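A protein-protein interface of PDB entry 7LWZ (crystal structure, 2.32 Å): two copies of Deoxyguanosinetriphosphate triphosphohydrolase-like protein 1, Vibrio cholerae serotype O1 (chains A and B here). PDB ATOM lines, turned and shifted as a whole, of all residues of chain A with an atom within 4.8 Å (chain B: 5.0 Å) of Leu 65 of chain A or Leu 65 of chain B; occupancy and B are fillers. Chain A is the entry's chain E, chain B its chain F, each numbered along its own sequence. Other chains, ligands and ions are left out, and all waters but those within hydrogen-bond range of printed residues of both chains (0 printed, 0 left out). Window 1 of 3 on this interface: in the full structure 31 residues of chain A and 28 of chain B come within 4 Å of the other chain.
Among the printed residues, 8 pairs touch across the chains.
The backbone NH of Leu 65 of chain B lies within hydrogen-bond range of the backbone carbonyl oxygen of Leu 46 of chain B, 3.2 Å away.
The side-chain hydroxyl of Thr 63 of chain B lies close to the backbone NH of Leu 65 of chain B, at 3.3 Å.
N of Thr 63 of chain B lies within hydrogen-bond range of OG1 of Thr 66 of chain B (2.9 Å).
The backbone carbonyl oxygen of Leu 46 of chain A sits at hydrogen-bond distance from the backbone NH of Leu 65 of chain A (3.1 Å).
The side-chain hydroxyl of Thr 63 of chain A lies close to the backbone NH of Leu 65 of chain A, 3.4 Å away.
The side-chain hydroxyl of Thr 63 of chain A lies within hydrogen-bond range of the backbone NH of Thr 66 of chain A, at 3.3 Å.
OE1 of Gln 47 of chain B sits at hydrogen-bond distance from OG1 of Thr 63 of chain A, 2.5 Å away.
NE2 of Gln 47 of chain B is in hydrogen-bond range of OG1 of Thr 66 of chain A (3.5 Å).
The side-chain hydroxyl (OG1) of Thr 63 of chain B is in hydrogen-bond range of the side-chain amide oxygen (OE1) of Gln 47 of chain A (2.5 Å).
Of the printed residues of chain B, Leu 65 of chain A touches Gln 47 (3.8 Å) and Leu 65 (3.95 Å).
Of the printed residues of chain B, Thr 63 of chain A touches Gln 47.
Of the printed residues of chain A, Thr 63 of chain B touches Gln 47 (2.5 Å).
Leu 69 of chain A touches none of the printed residues of chain B.
The nearest printed residue of chain B that does not touch Leu 65 of chain A is Leu 69 of chain B (5.4 Å).
The nearest printed residue of chain A that does not touch Leu 65 of chain B is Leu 69 of chain A (5.4 Å).
Gln 47 of chain A touches Gln 47 of chain B (CA to OE1, 3.5 Å).
Leu 65 of chain B touches Gln 47 of chain A.
NE2 of Gln 47 of chain A touches CG2 of Thr 66 of chain B, 3.2 Å away.
Gln 47 of chain B touches Leu 65 of chain A (OE1 to CB, 3.8 Å).
CD2 of Leu 65 of chain A touches CD2 of Leu 65 of chain B, 3.95 Å away.
Gln 47 of chain A touches its own counterpart, Gln 47 of chain B.
Gln 47 of chain A touches Leu 65 of chain B, and with the chains exchanged Leu 65 of chain A touches Gln 47 of chain B.
Gln 47 of chain A touches Thr 66 of chain B, and with the chains exchanged Thr 66 of chain A touches Gln 47 of chain B.
Leu 65 of chain A touches its own counterpart, Leu 65 of chain B.
Positions printed for both chains: 43, 46, 47, 63, 64, 65, 66, 67, 68 and 69.
Of the 8 pairs that touch across the chains among the printed residues, 8 have their exchanged pair printed and touching as well.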
ATOM      1  N   PHE A  43     -22.540 -10.849   0.727  1.00  0.00           N
ATOM      2  CA  PHE A  43     -22.991  -9.946  -0.315  1.00  0.00           C
ATOM      3  C   PHE A  43     -21.993  -9.935  -1.462  1.00  0.00           C
ATOM      4  O   PHE A  43     -22.382  -9.926  -2.635  1.00  0.00           O
ATOM      5  CB  PHE A  43     -23.203  -8.534   0.237  1.00  0.00           C
ATOM      6  CG  PHE A  43     -23.644  -7.544  -0.806  1.00  0.00           C
ATOM      7  CD1 PHE A  43     -24.939  -7.555  -1.289  1.00  0.00           C
ATOM      8  CD2 PHE A  43     -22.743  -6.641  -1.341  1.00  0.00           C
ATOM      9  CE1 PHE A  43     -25.349  -6.645  -2.255  1.00  0.00           C
ATOM     10  CE2 PHE A  43     -23.133  -5.723  -2.321  1.00  0.00           C
ATOM     11  CZ  PHE A  43     -24.437  -5.720  -2.774  1.00  0.00           C
ATOM     12  N   LEU A  46     -22.147 -12.415  -4.445  1.00  0.00           N
ATOM     13  CA  LEU A  46     -23.147 -12.236  -5.493  1.00  0.00           C
ATOM     14  C   LEU A  46     -22.549 -11.727  -6.788  1.00  0.00           C
ATOM     15  O   LEU A  46     -23.269 -11.673  -7.790  1.00  0.00           O
ATOM     16  CB  LEU A  46     -24.250 -11.297  -5.032  1.00  0.00           C
ATOM     17  CG  LEU A  46     -24.888 -11.702  -3.702  1.00  0.00           C
ATOM     18  CD1 LEU A  46     -25.816 -10.607  -3.324  1.00  0.00           C
ATOM     19  CD2 LEU A  46     -25.626 -13.039  -3.788  1.00  0.00           C
ATOM     20  N   GLN A  47     -21.289 -11.286  -6.773  1.00  0.00           N
ATOM     21  CA  GLN A  47     -20.616 -10.924  -8.014  1.00  0.00           C
ATOM     22  C   GLN A  47     -20.302 -12.149  -8.858  1.00  0.00           C
ATOM     23  O   GLN A  47     -20.124 -12.020 -10.074  1.00  0.00           O
ATOM     24  CB  GLN A  47     -19.326 -10.172  -7.726  1.00  0.00           C
ATOM     25  CG  GLN A  47     -19.547  -8.856  -7.065  1.00  0.00           C
ATOM     26  CD  GLN A  47     -18.253  -8.215  -6.630  1.00  0.00           C
ATOM     27  OE1 GLN A  47     -17.752  -7.295  -7.284  1.00  0.00           O
ATOM     28  NE2 GLN A  47     -17.712  -8.678  -5.504  1.00  0.00           N
ATOM     29  N   THR A  63     -25.237  -9.888 -12.811  1.00  0.00           N
ATOM     30  CA  THR A  63     -25.083 -10.925 -11.767  1.00  0.00           C
ATOM     31  C   THR A  63     -26.153 -10.739 -10.697  1.00  0.00           C
ATOM     32  O   THR A  63     -26.947  -9.797 -10.807  1.00  0.00           O
ATOM     33  CB  THR A  63     -23.719 -10.761 -11.099  1.00  0.00           C
ATOM     34  OG1 THR A  63     -23.717  -9.447 -10.546  1.00  0.00           O
ATOM     35  CG2 THR A  63     -22.574 -10.883 -12.075  1.00  0.00           C
ATOM     36  N   ARG A  64     -26.161 -11.624  -9.705  1.00  0.00           N
ATOM     37  CA  ARG A  64     -27.120 -11.506  -8.618  1.00  0.00           C
ATOM     38  C   ARG A  64     -26.909 -10.217  -7.835  1.00  0.00           C
ATOM     39  O   ARG A  64     -27.874  -9.651  -7.315  1.00  0.00           O
ATOM     40  CB  ARG A  64     -26.989 -12.714  -7.703  1.00  0.00           C
ATOM     41  CG  ARG A  64     -27.503 -14.007  -8.313  1.00  0.00           C
ATOM     42  CD  ARG A  64     -27.937 -14.957  -7.222  1.00  0.00           C
ATOM     43  NE  ARG A  64     -28.988 -15.864  -7.669  1.00  0.00           N
ATOM     44  CZ  ARG A  64     -28.881 -17.188  -7.661  1.00  0.00           C
ATOM     45  NH1 ARG A  64     -27.766 -17.768  -7.221  1.00  0.00           N
ATOM     46  NH2 ARG A  64     -29.897 -17.929  -8.079  1.00  0.00           N
ATOM     47  N   LEU A  65     -25.670  -9.708  -7.805  1.00  0.00           N
ATOM     48  CA  LEU A  65     -25.410  -8.409  -7.198  1.00  0.00           C
ATOM     49  C   LEU A  65     -26.074  -7.315  -8.006  1.00  0.00           C
ATOM     50  O   LEU A  65     -26.749  -6.445  -7.449  1.00  0.00           O
ATOM     51  CB  LEU A  65     -23.908  -8.136  -7.093  1.00  0.00           C
ATOM     52  CG  LEU A  65     -23.499  -6.828  -6.391  1.00  0.00           C
ATOM     53  CD1 LEU A  65     -22.390  -7.091  -5.401  1.00  0.00           C
ATOM     54  CD2 LEU A  65     -23.068  -5.747  -7.362  1.00  0.00           C
ATOM     55  N   THR A  66     -25.917  -7.371  -9.322  1.00  0.00           N
ATOM     56  CA  THR A  66     -26.577  -6.424 -10.210  1.00  0.00           C
ATOM     57  C   THR A  66     -28.087  -6.429 -10.026  1.00  0.00           C
ATOM     58  O   THR A  66     -28.701  -5.363  -9.964  1.00  0.00           O
ATOM     59  CB  THR A  66     -26.229  -6.772 -11.660  1.00  0.00           C
ATOM     60  OG1 THR A  66     -24.939  -6.234 -11.973  1.00  0.00           O
ATOM     61  CG2 THR A  66     -27.336  -6.302 -12.679  1.00  0.00           C
ATOM     62  N   HIS A  67     -28.703  -7.615  -9.945  1.00  0.00           N
ATOM     63  CA  HIS A  67     -30.143  -7.693  -9.708  1.00  0.00           C
ATOM     64  C   HIS A  67     -30.514  -7.040  -8.381  1.00  0.00           C
ATOM     65  O   HIS A  67     -31.484  -6.277  -8.308  1.00  0.00           O
ATOM     66  CB  HIS A  67     -30.601  -9.155  -9.772  1.00  0.00           C
ATOM     67  CG  HIS A  67     -31.858  -9.461  -9.011  1.00  0.00           C
ATOM     68  ND1 HIS A  67     -33.109  -9.129  -9.474  1.00  0.00           N
ATOM     69  CD2 HIS A  67     -32.057 -10.143  -7.855  1.00  0.00           C
ATOM     70  CE1 HIS A  67     -34.023  -9.565  -8.624  1.00  0.00           C
ATOM     71  NE2 HIS A  67     -33.413 -10.190  -7.634  1.00  0.00           N
ATOM     72  N   SER A  68     -29.702  -7.244  -7.344  1.00  0.00           N
ATOM     73  CA  SER A  68     -30.078  -6.710  -6.044  1.00  0.00           C
ATOM     74  C   SER A  68     -29.920  -5.197  -5.985  1.00  0.00           C
ATOM     75  O   SER A  68     -30.730  -4.531  -5.337  1.00  0.00           O
ATOM     76  CB  SER A  68     -29.263  -7.381  -4.942  1.00  0.00           C
ATOM     77  OG  SER A  68     -29.294  -8.795  -5.068  1.00  0.00           O
ATOM     78  N   LEU A  69     -28.964  -4.620  -6.719  1.00  0.00           N
ATOM     79  CA  LEU A  69     -28.896  -3.162  -6.779  1.00  0.00           C
ATOM     80  C   LEU A  69     -30.124  -2.601  -7.466  1.00  0.00           C
ATOM     81  O   LEU A  69     -30.686  -1.595  -7.019  1.00  0.00           O
ATOM     82  CB  LEU A  69     -27.635  -2.699  -7.513  1.00  0.00           C
ATOM     83  CG  LEU A  69     -26.337  -3.054  -6.800  1.00  0.00           C
ATOM     84  CD1 LEU A  69     -25.166  -2.579  -7.615  1.00  0.00           C
ATOM     85  CD2 LEU A  69     -26.314  -2.473  -5.385  1.00  0.00           C
ATOM     86  N   PHE B  43     -19.959   0.477 -14.910  1.00  0.00           N
ATOM     87  CA  PHE B  43     -19.937   0.132 -13.495  1.00  0.00           C
ATOM     88  C   PHE B  43     -20.046  -1.375 -13.290  1.00  0.00           C
ATOM     89  O   PHE B  43     -19.364  -1.929 -12.420  1.00  0.00           O
ATOM     90  CB  PHE B  43     -21.049   0.861 -12.740  1.00  0.00           C
ATOM     91  CG  PHE B  43     -21.083   0.544 -11.280  1.00  0.00           C
ATOM     92  CD1 PHE B  43     -20.149   1.109 -10.416  1.00  0.00           C
ATOM     93  CD2 PHE B  43     -22.022  -0.344 -10.776  1.00  0.00           C
ATOM     94  CE1 PHE B  43     -20.152   0.797  -9.074  1.00  0.00           C
ATOM     95  CE2 PHE B  43     -22.040  -0.660  -9.420  1.00  0.00           C
ATOM     96  CZ  PHE B  43     -21.099  -0.090  -8.570  1.00  0.00           C
ATOM     97  N   LEU B  46     -16.913  -3.649 -13.343  1.00  0.00           N
ATOM     98  CA  LEU B  46     -16.011  -3.646 -12.198  1.00  0.00           C
ATOM     99  C   LEU B  46     -16.066  -4.940 -11.398  1.00  0.00           C
ATOM    100  O   LEU B  46     -15.186  -5.164 -10.554  1.00  0.00           O
ATOM    101  CB  LEU B  46     -16.341  -2.472 -11.291  1.00  0.00           C
ATOM    102  CG  LEU B  46     -16.215  -1.112 -11.962  1.00  0.00           C
ATOM    103  CD1 LEU B  46     -16.858  -0.079 -11.076  1.00  0.00           C
ATOM    104  CD2 LEU B  46     -14.760  -0.779 -12.193  1.00  0.00           C
ATOM    105  N   GLN B  47     -17.081  -5.780 -11.639  1.00  0.00           N
ATOM    106  CA  GLN B  47     -17.173  -7.081 -10.985  1.00  0.00           C
ATOM    107  C   GLN B  47     -16.168  -8.091 -11.520  1.00  0.00           C
ATOM    108  O   GLN B  47     -15.853  -9.060 -10.820  1.00  0.00           O
ATOM    109  CB  GLN B  47     -18.572  -7.657 -11.147  1.00  0.00           C
ATOM    110  CG  GLN B  47     -19.664  -6.877 -10.445  1.00  0.00           C
ATOM    111  CD  GLN B  47     -21.029  -7.420 -10.792  1.00  0.00           C
ATOM    112  OE1 GLN B  47     -21.574  -8.233 -10.065  1.00  0.00           O
ATOM    113  NE2 GLN B  47     -21.566  -7.002 -11.929  1.00  0.00           N
ATOM    114  N   THR B  63     -13.175  -7.068  -5.581  1.00  0.00           N
ATOM    115  CA  THR B  63     -13.038  -6.583  -6.943  1.00  0.00           C
ATOM    116  C   THR B  63     -12.962  -5.063  -6.931  1.00  0.00           C
ATOM    117  O   THR B  63     -13.094  -4.424  -5.879  1.00  0.00           O
ATOM    118  CB  THR B  63     -14.222  -7.016  -7.808  1.00  0.00           C
ATOM    119  OG1 THR B  63     -15.416  -6.442  -7.267  1.00  0.00           O
ATOM    120  CG2 THR B  63     -14.362  -8.527  -7.828  1.00  0.00           C
ATOM    121  N   ARG B  64     -12.772  -4.468  -8.111  1.00  0.00           N
ATOM    122  CA  ARG B  64     -12.793  -3.014  -8.180  1.00  0.00           C
ATOM    123  C   ARG B  64     -14.155  -2.461  -7.773  1.00  0.00           C
ATOM    124  O   ARG B  64     -14.235  -1.356  -7.213  1.00  0.00           O
ATOM    125  CB  ARG B  64     -12.441  -2.544  -9.597  1.00  0.00           C
ATOM    126  CG  ARG B  64     -11.022  -2.900 -10.036  1.00  0.00           C
ATOM    127  CD  ARG B  64     -10.444  -1.829 -10.958  1.00  0.00           C
ATOM    128  NE  ARG B  64      -9.307  -2.291 -11.758  1.00  0.00           N
ATOM    129  CZ  ARG B  64      -8.052  -1.861 -11.618  1.00  0.00           C
ATOM    130  NH1 ARG B  64      -7.750  -0.952 -10.700  1.00  0.00           N
ATOM    131  NH2 ARG B  64      -7.092  -2.345 -12.397  1.00  0.00           N
ATOM    132  N   LEU B  65     -15.227  -3.236  -7.970  1.00  0.00           N
ATOM    133  CA  LEU B  65     -16.547  -2.782  -7.536  1.00  0.00           C
ATOM    134  C   LEU B  65     -16.636  -2.710  -6.008  1.00  0.00           C
ATOM    135  O   LEU B  65     -17.005  -1.675  -5.452  1.00  0.00           O
ATOM    136  CB  LEU B  65     -17.638  -3.695  -8.110  1.00  0.00           C
ATOM    137  CG  LEU B  65     -19.073  -3.347  -7.693  1.00  0.00           C
ATOM    138  CD1 LEU B  65     -20.023  -3.513  -8.875  1.00  0.00           C
ATOM    139  CD2 LEU B  65     -19.527  -4.199  -6.529  1.00  0.00           C
ATOM    140  N   THR B  66     -16.235  -3.773  -5.305  1.00  0.00           N
ATOM    141  CA  THR B  66     -16.243  -3.717  -3.845  1.00  0.00           C
ATOM    142  C   THR B  66     -15.311  -2.619  -3.305  1.00  0.00           C
ATOM    143  O   THR B  66     -15.657  -1.940  -2.334  1.00  0.00           O
ATOM    144  CB  THR B  66     -15.931  -5.087  -3.250  1.00  0.00           C
ATOM    145  OG1 THR B  66     -14.602  -5.467  -3.590  1.00  0.00           O
ATOM    146  CG2 THR B  66     -16.934  -6.115  -3.769  1.00  0.00           C
ATOM    147  N   HIS B  67     -14.136  -2.422  -3.912  1.00  0.00           N
ATOM    148  CA  HIS B  67     -13.291  -1.304  -3.506  1.00  0.00           C
ATOM    149  C   HIS B  67     -14.065  -0.002  -3.614  1.00  0.00           C
ATOM    150  O   HIS B  67     -14.011   0.839  -2.713  1.00  0.00           O
ATOM    151  CB  HIS B  67     -12.021  -1.256  -4.370  1.00  0.00           C
ATOM    152  CG  HIS B  67     -11.367   0.096  -4.476  1.00  0.00           C
ATOM    153  ND1 HIS B  67     -10.521   0.595  -3.508  1.00  0.00           N
ATOM    154  CD2 HIS B  67     -11.376   1.017  -5.471  1.00  0.00           C
ATOM    155  CE1 HIS B  67     -10.063   1.774  -3.891  1.00  0.00           C
ATOM    156  NE2 HIS B  67     -10.566   2.054  -5.079  1.00  0.00           N
ATOM    157  N   SER B  68     -14.860   0.144  -4.668  1.00  0.00           N
ATOM    158  CA  SER B  68     -15.542   1.410  -4.863  1.00  0.00           C
ATOM    159  C   SER B  68     -16.709   1.556  -3.894  1.00  0.00           C
ATOM    160  O   SER B  68     -17.028   2.679  -3.476  1.00  0.00           O
ATOM    161  CB  SER B  68     -16.002   1.555  -6.320  1.00  0.00           C
ATOM    162  OG  SER B  68     -14.962   1.203  -7.205  1.00  0.00           O
ATOM    163  N   LEU B  69     -17.317   0.443  -3.482  1.00  0.00           N
ATOM    164  CA  LEU B  69     -18.329   0.523  -2.436  1.00  0.00           C
ATOM    165  C   LEU B  69     -17.713   0.955  -1.111  1.00  0.00           C
ATOM    166  O   LEU B  69     -18.260   1.826  -0.417  1.00  0.00           O
ATOM    167  CB  LEU B  69     -19.047  -0.814  -2.298  1.00  0.00           C
ATOM    168  CG  LEU B  69     -20.065  -1.040  -3.425  1.00  0.00           C
ATOM    169  CD1 LEU B  69     -20.743  -2.381  -3.283  1.00  0.00           C
ATOM    170  CD2 LEU B  69     -21.090   0.075  -3.461  1.00  0.00           C
